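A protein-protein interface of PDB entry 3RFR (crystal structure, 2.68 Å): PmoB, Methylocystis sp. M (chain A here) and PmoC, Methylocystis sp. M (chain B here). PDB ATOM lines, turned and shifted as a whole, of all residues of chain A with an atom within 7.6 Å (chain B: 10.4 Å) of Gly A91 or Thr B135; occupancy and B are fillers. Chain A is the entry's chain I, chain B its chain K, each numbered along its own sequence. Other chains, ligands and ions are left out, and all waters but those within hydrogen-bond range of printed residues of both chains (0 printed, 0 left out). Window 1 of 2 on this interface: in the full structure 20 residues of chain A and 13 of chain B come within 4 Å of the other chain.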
ATOM      1  N   ALA A  87       8.375  12.711   2.583  1.00  0.00           N
ATOM      2  CA  ALA A  87       8.616  13.697   1.606  1.00  0.00           C
ATOM      3  C   ALA A  87       7.226  13.993   1.066  1.00  0.00           C
ATOM      4  O   ALA A  87       6.605  13.172   0.348  1.00  0.00           O
ATOM      5  CB  ALA A  87       9.489  13.105   0.556  1.00  0.00           C
ATOM      6  N   GLY A  88       6.710  15.166   1.401  1.00  0.00           N
ATOM      7  CA  GLY A  88       5.479  15.647   0.755  1.00  0.00           C
ATOM      8  C   GLY A  88       5.826  15.946  -0.677  1.00  0.00           C
ATOM      9  O   GLY A  88       6.770  16.653  -0.917  1.00  0.00           O
ATOM     10  N   GLU A  89       5.143  15.335  -1.618  1.00  0.00           N
ATOM     11  CA  GLU A  89       5.466  15.451  -3.039  1.00  0.00           C
ATOM     12  C   GLU A  89       4.351  14.806  -3.922  1.00  0.00           C
ATOM     13  O   GLU A  89       3.605  13.951  -3.463  1.00  0.00           O
ATOM     14  CB  GLU A  89       6.848  14.854  -3.390  1.00  0.00           C
ATOM     15  CG  GLU A  89       7.007  13.350  -3.140  1.00  0.00           C
ATOM     16  CD  GLU A  89       8.183  12.704  -3.895  1.00  0.00           C
ATOM     17  OE1 GLU A  89       8.743  13.358  -4.821  1.00  0.00           O
ATOM     18  OE2 GLU A  89       8.514  11.503  -3.585  1.00  0.00           O
ATOM     19  N   PRO A  90       4.206  15.266  -5.179  1.00  0.00           N
ATOM     20  CA  PRO A  90       3.016  14.765  -5.881  1.00  0.00           C
ATOM     21  C   PRO A  90       3.312  13.410  -6.488  1.00  0.00           C
ATOM     22  O   PRO A  90       3.619  13.325  -7.652  1.00  0.00           O
ATOM     23  CB  PRO A  90       2.812  15.828  -6.992  1.00  0.00           C
ATOM     24  CG  PRO A  90       4.217  16.455  -7.196  1.00  0.00           C
ATOM     25  CD  PRO A  90       4.820  16.468  -5.837  1.00  0.00           C
ATOM     26  N   GLY A  91       3.231  12.344  -5.711  1.00  0.00           N
ATOM     27  CA  GLY A  91       3.561  10.987  -6.238  1.00  0.00           C
ATOM     28  C   GLY A  91       5.078  10.806  -6.334  1.00  0.00           C
ATOM     29  O   GLY A  91       5.859  11.656  -5.885  1.00  0.00           O
ATOM     30  N   PRO A  92       5.525   9.710  -6.909  1.00  0.00           N
ATOM     31  CA  PRO A  92       6.960   9.514  -6.768  1.00  0.00           C
ATOM     32  C   PRO A  92       7.723  10.249  -7.871  1.00  0.00           C
ATOM     33  O   PRO A  92       8.288   9.569  -8.766  1.00  0.00           O
ATOM     34  CB  PRO A  92       7.126   7.945  -6.852  1.00  0.00           C
ATOM     35  CG  PRO A  92       5.900   7.450  -7.502  1.00  0.00           C
ATOM     36  CD  PRO A  92       4.805   8.502  -7.353  1.00  0.00           C
ATOM     37  N   VAL A  93       7.701  11.605  -7.862  1.00  0.00           N
ATOM     38  CA  VAL A  93       8.487  12.379  -8.824  1.00  0.00           C
ATOM     39  C   VAL A  93       9.958  12.252  -8.465  1.00  0.00           C
ATOM     40  O   VAL A  93      10.790  12.104  -9.374  1.00  0.00           O
ATOM     41  CB  VAL A  93       8.049  13.884  -9.041  1.00  0.00           C
ATOM     42  CG1 VAL A  93       6.618  14.011  -9.709  1.00  0.00           C
ATOM     43  CG2 VAL A  93       8.159  14.690  -7.782  1.00  0.00           C
ATOM     44  N   LEU A  94      10.291  12.316  -7.167  1.00  0.00           N
ATOM     45  CA  LEU A  94      11.562  11.765  -6.661  1.00  0.00           C
ATOM     46  C   LEU A  94      11.297  10.460  -5.855  1.00  0.00           C
ATOM     47  O   LEU A  94      10.335  10.381  -5.067  1.00  0.00           O
ATOM     48  CB  LEU A  94      12.316  12.762  -5.788  1.00  0.00           C
ATOM     49  CG  LEU A  94      12.725  14.097  -6.478  1.00  0.00           C
ATOM     50  CD1 LEU A  94      11.894  15.310  -6.054  1.00  0.00           C
ATOM     51  CD2 LEU A  94      14.233  14.411  -6.273  1.00  0.00           C
ATOM     52  N   VAL A  95      12.176   9.466  -6.049  1.00  0.00           N
ATOM     53  CA  VAL A  95      12.191   8.213  -5.265  1.00  0.00           C
ATOM     54  C   VAL A  95      12.966   8.400  -3.958  1.00  0.00           C
ATOM     55  O   VAL A  95      14.102   8.846  -3.956  1.00  0.00           O
ATOM     56  CB  VAL A  95      12.793   7.053  -6.137  1.00  0.00           C
ATOM     57  CG1 VAL A  95      13.542   5.994  -5.328  1.00  0.00           C
ATOM     58  CG2 VAL A  95      11.699   6.417  -6.996  1.00  0.00           C
ATOM     59  N   ARG A 127      13.246  11.215 -10.712  1.00  0.00           N
ATOM     60  CA  ARG A 127      12.499  10.187 -11.443  1.00  0.00           C
ATOM     61  C   ARG A 127      11.649  10.796 -12.576  1.00  0.00           C
ATOM     62  O   ARG A 127      11.844  10.448 -13.736  1.00  0.00           O
ATOM     63  CB  ARG A 127      11.682   9.273 -10.490  1.00  0.00           C
ATOM     64  CG  ARG A 127      10.826   8.197 -11.170  1.00  0.00           C
ATOM     65  CD  ARG A 127      10.355   7.072 -10.128  1.00  0.00           C
ATOM     66  NE  ARG A 127       9.632   5.968 -10.778  1.00  0.00           N
ATOM     67  CZ  ARG A 127       8.308   5.891 -10.900  1.00  0.00           C
ATOM     68  NH1 ARG A 127       7.772   4.870 -11.573  1.00  0.00           N
ATOM     69  NH2 ARG A 127       7.520   6.824 -10.344  1.00  0.00           N
ATOM     70  N   ARG A 128      10.727  11.694 -12.281  1.00  0.00           N
ATOM     71  CA  ARG A 128       9.982  12.346 -13.374  1.00  0.00           C
ATOM     72  C   ARG A 128      10.349  13.804 -13.666  1.00  0.00           C
ATOM     73  O   ARG A 128      10.231  14.628 -12.772  1.00  0.00           O
ATOM     74  CB  ARG A 128       8.515  12.364 -13.037  1.00  0.00           C
ATOM     75  CG  ARG A 128       7.711  11.288 -13.599  1.00  0.00           C
ATOM     76  CD  ARG A 128       6.369  11.464 -12.987  1.00  0.00           C
ATOM     77  NE  ARG A 128       5.501  12.262 -13.838  1.00  0.00           N
ATOM     78  CZ  ARG A 128       4.476  12.972 -13.379  1.00  0.00           C
ATOM     79  NH1 ARG A 128       3.700  13.628 -14.224  1.00  0.00           N
ATOM     80  NH2 ARG A 128       4.211  13.015 -12.067  1.00  0.00           N
ATOM     81  N   TRP A 132       8.511  20.802  -9.043  1.00  0.00           N
ATOM     82  CA  TRP A 132       7.708  20.075  -8.045  1.00  0.00           C
ATOM     83  C   TRP A 132       7.981  20.634  -6.668  1.00  0.00           C
ATOM     84  O   TRP A 132       9.125  21.038  -6.374  1.00  0.00           O
ATOM     85  CB  TRP A 132       8.024  18.562  -8.030  1.00  0.00           C
ATOM     86  CG  TRP A 132       8.036  17.838  -9.348  1.00  0.00           C
ATOM     87  CD1 TRP A 132       9.130  17.337  -9.982  1.00  0.00           C
ATOM     88  CD2 TRP A 132       6.917  17.480 -10.154  1.00  0.00           C
ATOM     89  NE1 TRP A 132       8.770  16.678 -11.133  1.00  0.00           N
ATOM     90  CE2 TRP A 132       7.413  16.748 -11.266  1.00  0.00           C
ATOM     91  CE3 TRP A 132       5.536  17.699 -10.055  1.00  0.00           C
ATOM     92  CZ2 TRP A 132       6.573  16.238 -12.282  1.00  0.00           C
ATOM     93  CZ3 TRP A 132       4.689  17.199 -11.075  1.00  0.00           C
ATOM     94  CH2 TRP A 132       5.223  16.480 -12.178  1.00  0.00           C
ATOM     95  N   VAL A 134       8.494  19.997  -2.988  1.00  0.00           N
ATOM     96  CA  VAL A 134       8.842  18.931  -2.124  1.00  0.00           C
ATOM     97  C   VAL A 134       9.025  19.432  -0.690  1.00  0.00           C
ATOM     98  O   VAL A 134      10.035  20.084  -0.358  1.00  0.00           O
ATOM     99  CB  VAL A 134      10.081  18.161  -2.627  1.00  0.00           C
ATOM    100  CG1 VAL A 134      10.345  16.953  -1.723  1.00  0.00           C
ATOM    101  CG2 VAL A 134       9.829  17.626  -4.021  1.00  0.00           C
ATOM    102  N   GLU B  42      -7.710  14.912 -17.593  1.00  0.00           N
ATOM    103  CA  GLU B  42      -7.113  14.850 -16.258  1.00  0.00           C
ATOM    104  C   GLU B  42      -5.612  14.474 -16.245  1.00  0.00           C
ATOM    105  O   GLU B  42      -4.833  15.010 -15.455  1.00  0.00           O
ATOM    106  CB  GLU B  42      -7.972  14.058 -15.263  1.00  0.00           C
ATOM    107  CG  GLU B  42      -8.361  12.653 -15.719  1.00  0.00           C
ATOM    108  CD  GLU B  42      -9.301  11.907 -14.756  1.00  0.00           C
ATOM    109  OE1 GLU B  42      -9.901  12.503 -13.823  1.00  0.00           O
ATOM    110  OE2 GLU B  42      -9.435  10.684 -14.954  1.00  0.00           O
ATOM    111  N   PHE B  45      -4.271  18.173 -17.257  1.00  0.00           N
ATOM    112  CA  PHE B  45      -4.497  19.241 -16.280  1.00  0.00           C
ATOM    113  C   PHE B  45      -4.563  18.727 -14.856  1.00  0.00           C
ATOM    114  O   PHE B  45      -4.736  19.507 -13.921  1.00  0.00           O
ATOM    115  CB  PHE B  45      -5.772  20.015 -16.597  1.00  0.00           C
ATOM    116  CG  PHE B  45      -5.731  20.730 -17.898  1.00  0.00           C
ATOM    117  CD1 PHE B  45      -5.098  21.962 -18.004  1.00  0.00           C
ATOM    118  CD2 PHE B  45      -6.320  20.181 -19.027  1.00  0.00           C
ATOM    119  CE1 PHE B  45      -5.047  22.635 -19.217  1.00  0.00           C
ATOM    120  CE2 PHE B  45      -6.277  20.860 -20.253  1.00  0.00           C
ATOM    121  CZ  PHE B  45      -5.640  22.083 -20.342  1.00  0.00           C
ATOM    122  N   GLY B  46      -4.437  17.415 -14.689  1.00  0.00           N
ATOM    123  CA  GLY B  46      -4.197  16.840 -13.370  1.00  0.00           C
ATOM    124  C   GLY B  46      -2.960  17.483 -12.781  1.00  0.00           C
ATOM    125  O   GLY B  46      -3.028  18.084 -11.710  1.00  0.00           O
ATOM    126  N   TRP B  47      -1.837  17.381 -13.497  1.00  0.00           N
ATOM    127  CA  TRP B  47      -0.639  18.142 -13.145  1.00  0.00           C
ATOM    128  C   TRP B  47      -0.603  19.546 -13.734  1.00  0.00           C
ATOM    129  O   TRP B  47      -1.071  19.812 -14.846  1.00  0.00           O
ATOM    130  CB  TRP B  47       0.626  17.376 -13.503  1.00  0.00           C
ATOM    131  CG  TRP B  47       0.849  16.262 -12.531  1.00  0.00           C
ATOM    132  CD1 TRP B  47       1.469  16.334 -11.310  1.00  0.00           C
ATOM    133  CD2 TRP B  47       0.413  14.915 -12.678  1.00  0.00           C
ATOM    134  NE1 TRP B  47       1.461  15.094 -10.693  1.00  0.00           N
ATOM    135  CE2 TRP B  47       0.816  14.211 -11.507  1.00  0.00           C
ATOM    136  CE3 TRP B  47      -0.276  14.233 -13.682  1.00  0.00           C
ATOM    137  CZ2 TRP B  47       0.557  12.876 -11.321  1.00  0.00           C
ATOM    138  CZ3 TRP B  47      -0.529  12.914 -13.503  1.00  0.00           C
ATOM    139  CH2 TRP B  47      -0.116  12.235 -12.323  1.00  0.00           C
ATOM    140  N   ARG B  48      -0.042  20.460 -12.965  1.00  0.00           N
ATOM    141  CA  ARG B  48      -0.003  21.862 -13.384  1.00  0.00           C
ATOM    142  C   ARG B  48      -1.405  22.356 -13.683  1.00  0.00           C
ATOM    143  O   ARG B  48      -1.674  22.812 -14.778  1.00  0.00           O
ATOM    144  CB  ARG B  48       0.927  22.081 -14.614  1.00  0.00           C
ATOM    145  CG  ARG B  48       2.490  21.831 -14.424  1.00  0.00           C
ATOM    146  CD  ARG B  48       3.125  22.615 -13.269  1.00  0.00           C
ATOM    147  NE  ARG B  48       3.096  21.843 -12.020  1.00  0.00           N
ATOM    148  CZ  ARG B  48       3.337  22.339 -10.805  1.00  0.00           C
ATOM    149  NH1 ARG B  48       3.636  23.625 -10.637  1.00  0.00           N
ATOM    150  NH2 ARG B  48       3.279  21.538  -9.746  1.00  0.00           N
ATOM    151  N   GLY B  50      -4.256  20.957 -11.148  1.00  0.00           N
ATOM    152  CA  GLY B  50      -5.043  20.300 -10.110  1.00  0.00           C
ATOM    153  C   GLY B  50      -4.378  19.913  -8.802  1.00  0.00           C
ATOM    154  O   GLY B  50      -5.014  19.279  -7.956  1.00  0.00           O
ATOM    155  N   LEU B  51      -3.111  20.292  -8.624  1.00  0.00           N
ATOM    156  CA  LEU B  51      -2.358  19.946  -7.403  1.00  0.00           C
ATOM    157  C   LEU B  51      -2.574  20.939  -6.261  1.00  0.00           C
ATOM    158  O   LEU B  51      -2.458  20.578  -5.088  1.00  0.00           O
ATOM    159  CB  LEU B  51      -0.864  19.821  -7.696  1.00  0.00           C
ATOM    160  CG  LEU B  51      -0.360  18.753  -8.672  1.00  0.00           C
ATOM    161  CD1 LEU B  51       1.116  18.976  -8.939  1.00  0.00           C
ATOM    162  CD2 LEU B  51      -0.605  17.367  -8.160  1.00  0.00           C
ATOM    163  N   ASP B  52      -2.890  22.183  -6.607  1.00  0.00           N
ATOM    164  CA  ASP B  52      -3.049  23.245  -5.621  1.00  0.00           C
ATOM    165  C   ASP B  52      -4.355  23.938  -5.876  1.00  0.00           C
ATOM    166  O   ASP B  52      -4.499  24.691  -6.850  1.00  0.00           O
ATOM    167  CB  ASP B  52      -1.898  24.251  -5.721  1.00  0.00           C
ATOM    168  CG  ASP B  52      -2.158  25.559  -4.960  1.00  0.00           C
ATOM    169  OD1 ASP B  52      -3.101  25.628  -4.135  1.00  0.00           O
ATOM    170  OD2 ASP B  52      -1.389  26.523  -5.197  1.00  0.00           O
ATOM    171  N   GLU B 127     -11.930   3.938  -8.132  1.00  0.00           N
ATOM    172  CA  GLU B 127     -10.607   3.461  -7.722  1.00  0.00           C
ATOM    173  C   GLU B 127      -9.540   4.424  -8.215  1.00  0.00           C
ATOM    174  O   GLU B 127      -8.451   4.482  -7.696  1.00  0.00           O
ATOM    175  CB  GLU B 127     -10.322   2.013  -8.159  1.00  0.00           C
ATOM    176  CG  GLU B 127      -9.256   1.361  -7.273  1.00  0.00           C
ATOM    177  CD  GLU B 127      -8.891  -0.091  -7.608  1.00  0.00           C
ATOM    178  OE1 GLU B 127      -9.335  -1.016  -6.910  1.00  0.00           O
ATOM    179  OE2 GLU B 127      -8.117  -0.319  -8.550  1.00  0.00           O
ATOM    180  N   GLN B 128      -9.856   5.201  -9.224  1.00  0.00           N
ATOM    181  CA  GLN B 128      -8.953   6.252  -9.619  1.00  0.00           C
ATOM    182  C   GLN B 128      -8.732   7.206  -8.458  1.00  0.00           C
ATOM    183  O   GLN B 128      -7.605   7.645  -8.233  1.00  0.00           O
ATOM    184  CB  GLN B 128      -9.478   7.021 -10.820  1.00  0.00           C
ATOM    185  CG  GLN B 128      -8.649   8.227 -11.091  1.00  0.00           C
ATOM    186  CD  GLN B 128      -8.957   8.846 -12.414  1.00  0.00           C
ATOM    187  OE1 GLN B 128      -9.680   9.856 -12.485  1.00  0.00           O
ATOM    188  NE2 GLN B 128      -8.418   8.253 -13.496  1.00  0.00           N
ATOM    189  N   ASP B 129      -9.788   7.527  -7.717  1.00  0.00           N
ATOM    190  CA  ASP B 129      -9.650   8.347  -6.503  1.00  0.00           C
ATOM    191  C   ASP B 129      -8.601   7.771  -5.535  1.00  0.00           C
ATOM    192  O   ASP B 129      -7.883   8.514  -4.865  1.00  0.00           O
ATOM    193  CB  ASP B 129     -11.016   8.528  -5.826  1.00  0.00           C
ATOM    194  CG  ASP B 129     -10.998   9.541  -4.687  1.00  0.00           C
ATOM    195  OD1 ASP B 129     -10.694  10.744  -4.948  1.00  0.00           O
ATOM    196  OD2 ASP B 129     -11.310   9.127  -3.530  1.00  0.00           O
ATOM    197  N   GLY B 130      -8.488   6.441  -5.509  1.00  0.00           N
ATOM    198  CA  GLY B 130      -7.544   5.724  -4.643  1.00  0.00           C
ATOM    199  C   GLY B 130      -6.114   6.189  -4.795  1.00  0.00           C
ATOM    200  O   GLY B 130      -5.453   6.530  -3.813  1.00  0.00           O
ATOM    201  N   ALA B 131      -5.640   6.186  -6.041  1.00  0.00           N
ATOM    202  CA  ALA B 131      -4.287   6.676  -6.371  1.00  0.00           C
ATOM    203  C   ALA B 131      -4.120   8.197  -6.159  1.00  0.00           C
ATOM    204  O   ALA B 131      -3.038   8.624  -5.790  1.00  0.00           O
ATOM    205  CB  ALA B 131      -3.851   6.243  -7.824  1.00  0.00           C
ATOM    206  N   TRP B 132      -5.174   8.996  -6.362  1.00  0.00           N
ATOM    207  CA  TRP B 132      -5.050  10.455  -6.145  1.00  0.00           C
ATOM    208  C   TRP B 132      -4.902  10.842  -4.675  1.00  0.00           C
ATOM    209  O   TRP B 132      -4.214  11.801  -4.345  1.00  0.00           O
ATOM    210  CB  TRP B 132      -6.218  11.212  -6.744  1.00  0.00           C
ATOM    211  CG  TRP B 132      -5.976  12.703  -6.912  1.00  0.00           C
ATOM    212  CD1 TRP B 132      -6.573  13.715  -6.203  1.00  0.00           C
ATOM    213  CD2 TRP B 132      -5.122  13.340  -7.872  1.00  0.00           C
ATOM    214  NE1 TRP B 132      -6.142  14.929  -6.658  1.00  0.00           N
ATOM    215  CE2 TRP B 132      -5.255  14.743  -7.682  1.00  0.00           C
ATOM    216  CE3 TRP B 132      -4.254  12.870  -8.865  1.00  0.00           C
ATOM    217  CZ2 TRP B 132      -4.539  15.693  -8.449  1.00  0.00           C
ATOM    218  CZ3 TRP B 132      -3.539  13.809  -9.631  1.00  0.00           C
ATOM    219  CH2 TRP B 132      -3.684  15.213  -9.410  1.00  0.00           C
ATOM    220  N   HIS B 133      -5.547  10.085  -3.804  1.00  0.00           N
ATOM    221  CA  HIS B 133      -5.361  10.244  -2.376  1.00  0.00           C
ATOM    222  C   HIS B 133      -3.896  10.067  -1.948  1.00  0.00           C
ATOM    223  O   HIS B 133      -3.494  10.534  -0.893  1.00  0.00           O
ATOM    224  CB  HIS B 133      -6.291   9.285  -1.606  1.00  0.00           C
ATOM    225  CG  HIS B 133      -7.693   9.786  -1.479  1.00  0.00           C
ATOM    226  ND1 HIS B 133      -8.067  10.719  -0.532  1.00  0.00           N
ATOM    227  CD2 HIS B 133      -8.807   9.512  -2.195  1.00  0.00           C
ATOM    228  CE1 HIS B 133      -9.351  11.002  -0.673  1.00  0.00           C
ATOM    229  NE2 HIS B 133      -9.828  10.277  -1.672  1.00  0.00           N
ATOM    230  N   MET B 134      -3.098   9.402  -2.770  1.00  0.00           N
ATOM    231  CA  MET B 134      -1.697   9.179  -2.427  1.00  0.00           C
ATOM    232  C   MET B 134      -0.817  10.186  -3.144  1.00  0.00           C
ATOM    233  O   MET B 134       0.403  10.117  -3.053  1.00  0.00           O
ATOM    234  CB  MET B 134      -1.270   7.737  -2.733  1.00  0.00           C
ATOM    235  CG  MET B 134      -2.042   6.688  -1.952  1.00  0.00           C
ATOM    236  SD  MET B 134      -1.807   6.802  -0.181  1.00  0.00           S
ATOM    237  CE  MET B 134      -3.511   6.872   0.383  1.00  0.00           C
ATOM    238  N   THR B 135      -1.450  11.147  -3.818  1.00  0.00           N
ATOM    239  CA  THR B 135      -0.747  12.153  -4.585  1.00  0.00           C
ATOM    240  C   THR B 135      -0.773  13.510  -3.923  1.00  0.00           C
ATOM    241  O   THR B 135       0.210  14.260  -3.971  1.00  0.00           O
ATOM    242  CB  THR B 135      -1.332  12.273  -5.995  1.00  0.00           C
ATOM    243  OG1 THR B 135      -0.970  11.108  -6.734  1.00  0.00           O
ATOM    244  CG2 THR B 135      -0.799  13.539  -6.748  1.00  0.00           C
ATOM    245  N   VAL B 136      -1.899  13.840  -3.314  1.00  0.00           N
ATOM    246  CA  VAL B 136      -2.042  15.148  -2.685  1.00  0.00           C
ATOM    247  C   VAL B 136      -2.290  15.029  -1.190  1.00  0.00           C
ATOM    248  O   VAL B 136      -2.560  13.929  -0.689  1.00  0.00           O
ATOM    249  CB  VAL B 136      -3.199  15.915  -3.314  1.00  0.00           C
ATOM    250  CG1 VAL B 136      -2.882  16.249  -4.783  1.00  0.00           C
ATOM    251  CG2 VAL B 136      -4.495  15.101  -3.171  1.00  0.00           C
ATOM    252  N   ILE B 137      -2.212  16.159  -0.485  1.00  0.00           N
ATOM    253  CA  ILE B 137      -2.711  16.208   0.890  1.00  0.00           C
ATOM    254  C   ILE B 137      -4.088  16.912   1.018  1.00  0.00           C
ATOM    255  O   ILE B 137      -4.613  17.033   2.109  1.00  0.00           O
ATOM    256  CB  ILE B 137      -1.635  16.712   1.888  1.00  0.00           C
ATOM    257  CG1 ILE B 137      -0.366  15.871   1.750  1.00  0.00           C
ATOM    258  CG2 ILE B 137      -2.093  16.544   3.303  1.00  0.00           C
ATOM    259  CD1 ILE B 137       0.955  16.668   1.750  1.00  0.00           C
ATOM    260  N   ARG B 138      -4.671  17.323  -0.108  1.00  0.00           N
ATOM    261  CA  ARG B 138      -6.050  17.863  -0.221  1.00  0.00           C
ATOM    262  C   ARG B 138      -6.237  19.293   0.320  1.00  0.00           C
ATOM    263  O   ARG B 138      -6.254  19.506   1.524  1.00  0.00           O
ATOM    264  CB  ARG B 138      -7.100  16.876   0.335  1.00  0.00           C
ATOM    265  CG  ARG B 138      -7.233  15.592  -0.485  1.00  0.00           C
ATOM    266  CD  ARG B 138      -8.270  14.620   0.062  1.00  0.00           C
ATOM    267  NE  ARG B 138      -9.637  14.996  -0.294  1.00  0.00           N
ATOM    268  CZ  ARG B 138     -10.563  15.394   0.582  1.00  0.00           C
ATOM    269  NH1 ARG B 138     -11.784  15.723   0.166  1.00  0.00           N
ATOM    270  NH2 ARG B 138     -10.275  15.463   1.882  1.00  0.00           N
ATOM    271  N   ASP B 139      -6.372  20.271  -0.577  1.00  0.00           N
ATOM    272  CA  ASP B 139      -6.674  21.656  -0.180  1.00  0.00           C
ATOM    273  C   ASP B 139      -8.166  21.752   0.196  1.00  0.00           C
ATOM    274  O   ASP B 139      -8.583  22.657   0.930  1.00  0.00           O
ATOM    275  CB  ASP B 139      -6.419  22.689  -1.320  1.00  0.00           C
ATOM    276  CG  ASP B 139      -5.028  22.575  -2.016  1.00  0.00           C
ATOM    277  OD1 ASP B 139      -4.128  23.408  -1.717  1.00  0.00           O
ATOM    278  OD2 ASP B 139      -4.857  21.705  -2.914  1.00  0.00           O
ATOM    279  N   THR B 143     -11.357  17.731  -5.172  1.00  0.00           N
ATOM    280  CA  THR B 143     -10.156  17.384  -5.927  1.00  0.00           C
ATOM    281  C   THR B 143     -10.548  16.972  -7.352  1.00  0.00           C
ATOM    282  O   THR B 143     -11.683  16.521  -7.560  1.00  0.00           O
ATOM    283  CB  THR B 143      -9.363  16.253  -5.245  1.00  0.00           C
ATOM    284  OG1 THR B 143     -10.175  15.070  -5.108  1.00  0.00           O
ATOM    285  CG2 THR B 143      -8.863  16.701  -3.895  1.00  0.00           C
ATOM    286  N   PRO B 144      -9.625  17.110  -8.343  1.00  0.00           N
ATOM    287  CA  PRO B 144      -9.998  16.726  -9.719  1.00  0.00           C
ATOM    288  C   PRO B 144     -10.619  15.328  -9.756  1.00  0.00           C
ATOM    289  O   PRO B 144     -11.554  15.088 -10.512  1.00  0.00           O
ATOM    290  CB  PRO B 144      -8.662  16.719 -10.470  1.00  0.00           C
ATOM    291  CG  PRO B 144      -7.752  17.527  -9.682  1.00  0.00           C
ATOM    292  CD  PRO B 144      -8.193  17.465  -8.252  1.00  0.00           C
ATOM    293  N   SER B 145     -10.099  14.429  -8.929  1.00  0.00           N
ATOM    294  CA  SER B 145     -10.630  13.095  -8.773  1.00  0.00           C
ATOM    295  C   SER B 145     -12.108  13.080  -8.385  1.00  0.00           C
ATOM    296  O   SER B 145     -12.921  12.499  -9.090  1.00  0.00           O
ATOM    297  CB  SER B 145      -9.832  12.391  -7.709  1.00  0.00           C
ATOM    298  OG  SER B 145      -9.655  11.058  -8.095  1.00  0.00           O
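Of chain A, only Glu A89, Pro A90 and Gly A91 come within 4 Å of Thr B135.
Of chain B, only Thr B135 (3.4 Å) comes within 4 Å of Glu A89.
No residue of chain B comes within 4 Å of Pro A92.
Of the printed residues of chain B, Pro A90 touches Leu B51 and Thr B135.
Of the printed residues of chain A, Trp B47 touches Arg A128 and Trp A132.
Of the printed residues of chain B, Trp A132 touches Trp B47.
Printed residues of chain B within 4 Å of Arg A128: Trp B47 (3.6 Å).
Printed residues of chain A within 4 Å of Leu B51: Pro A90 (3.9 Å).
The nearest residue of chain B that does not touch Gly A91 is Met B134 (4.5 Å).
The side-chain carboxylate of Glu A89 sits at hydrogen-bond distance from the backbone NH of Leu A94 (3.0 Å).
The backbone NH (N) of Arg A128 sits at hydrogen-bond distance from the backbone carbonyl oxygen (O) of Val A93, at 2.9 Å.
O of Arg A128 is in hydrogen-bond range of NE1 of Trp A132 (3.0 Å).
The backbone carbonyl oxygen (O) of Ala B131 sits at hydrogen-bond distance from the side-chain hydroxyl (OG1) of Thr B135 (3.4 Å).
Of the 13 printed residues of chain A, 5 touch a printed residue of chain B.
Hydrophobic or aromatic side chains of chain B within 4 Å of the printed part of chain A: Trp B47 and Leu B51.
Among the printed residues, 6 pairs touch across the chains.
O of Glu A89 lies close to O of Thr B135.
Among the printed residues, merely in contact across the chains: Pro A90 with Leu B51, Pro A90 with Thr B135, Gly A91 with Thr B135, Arg A128 with Trp B47 and Trp A132 with Trp B47.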
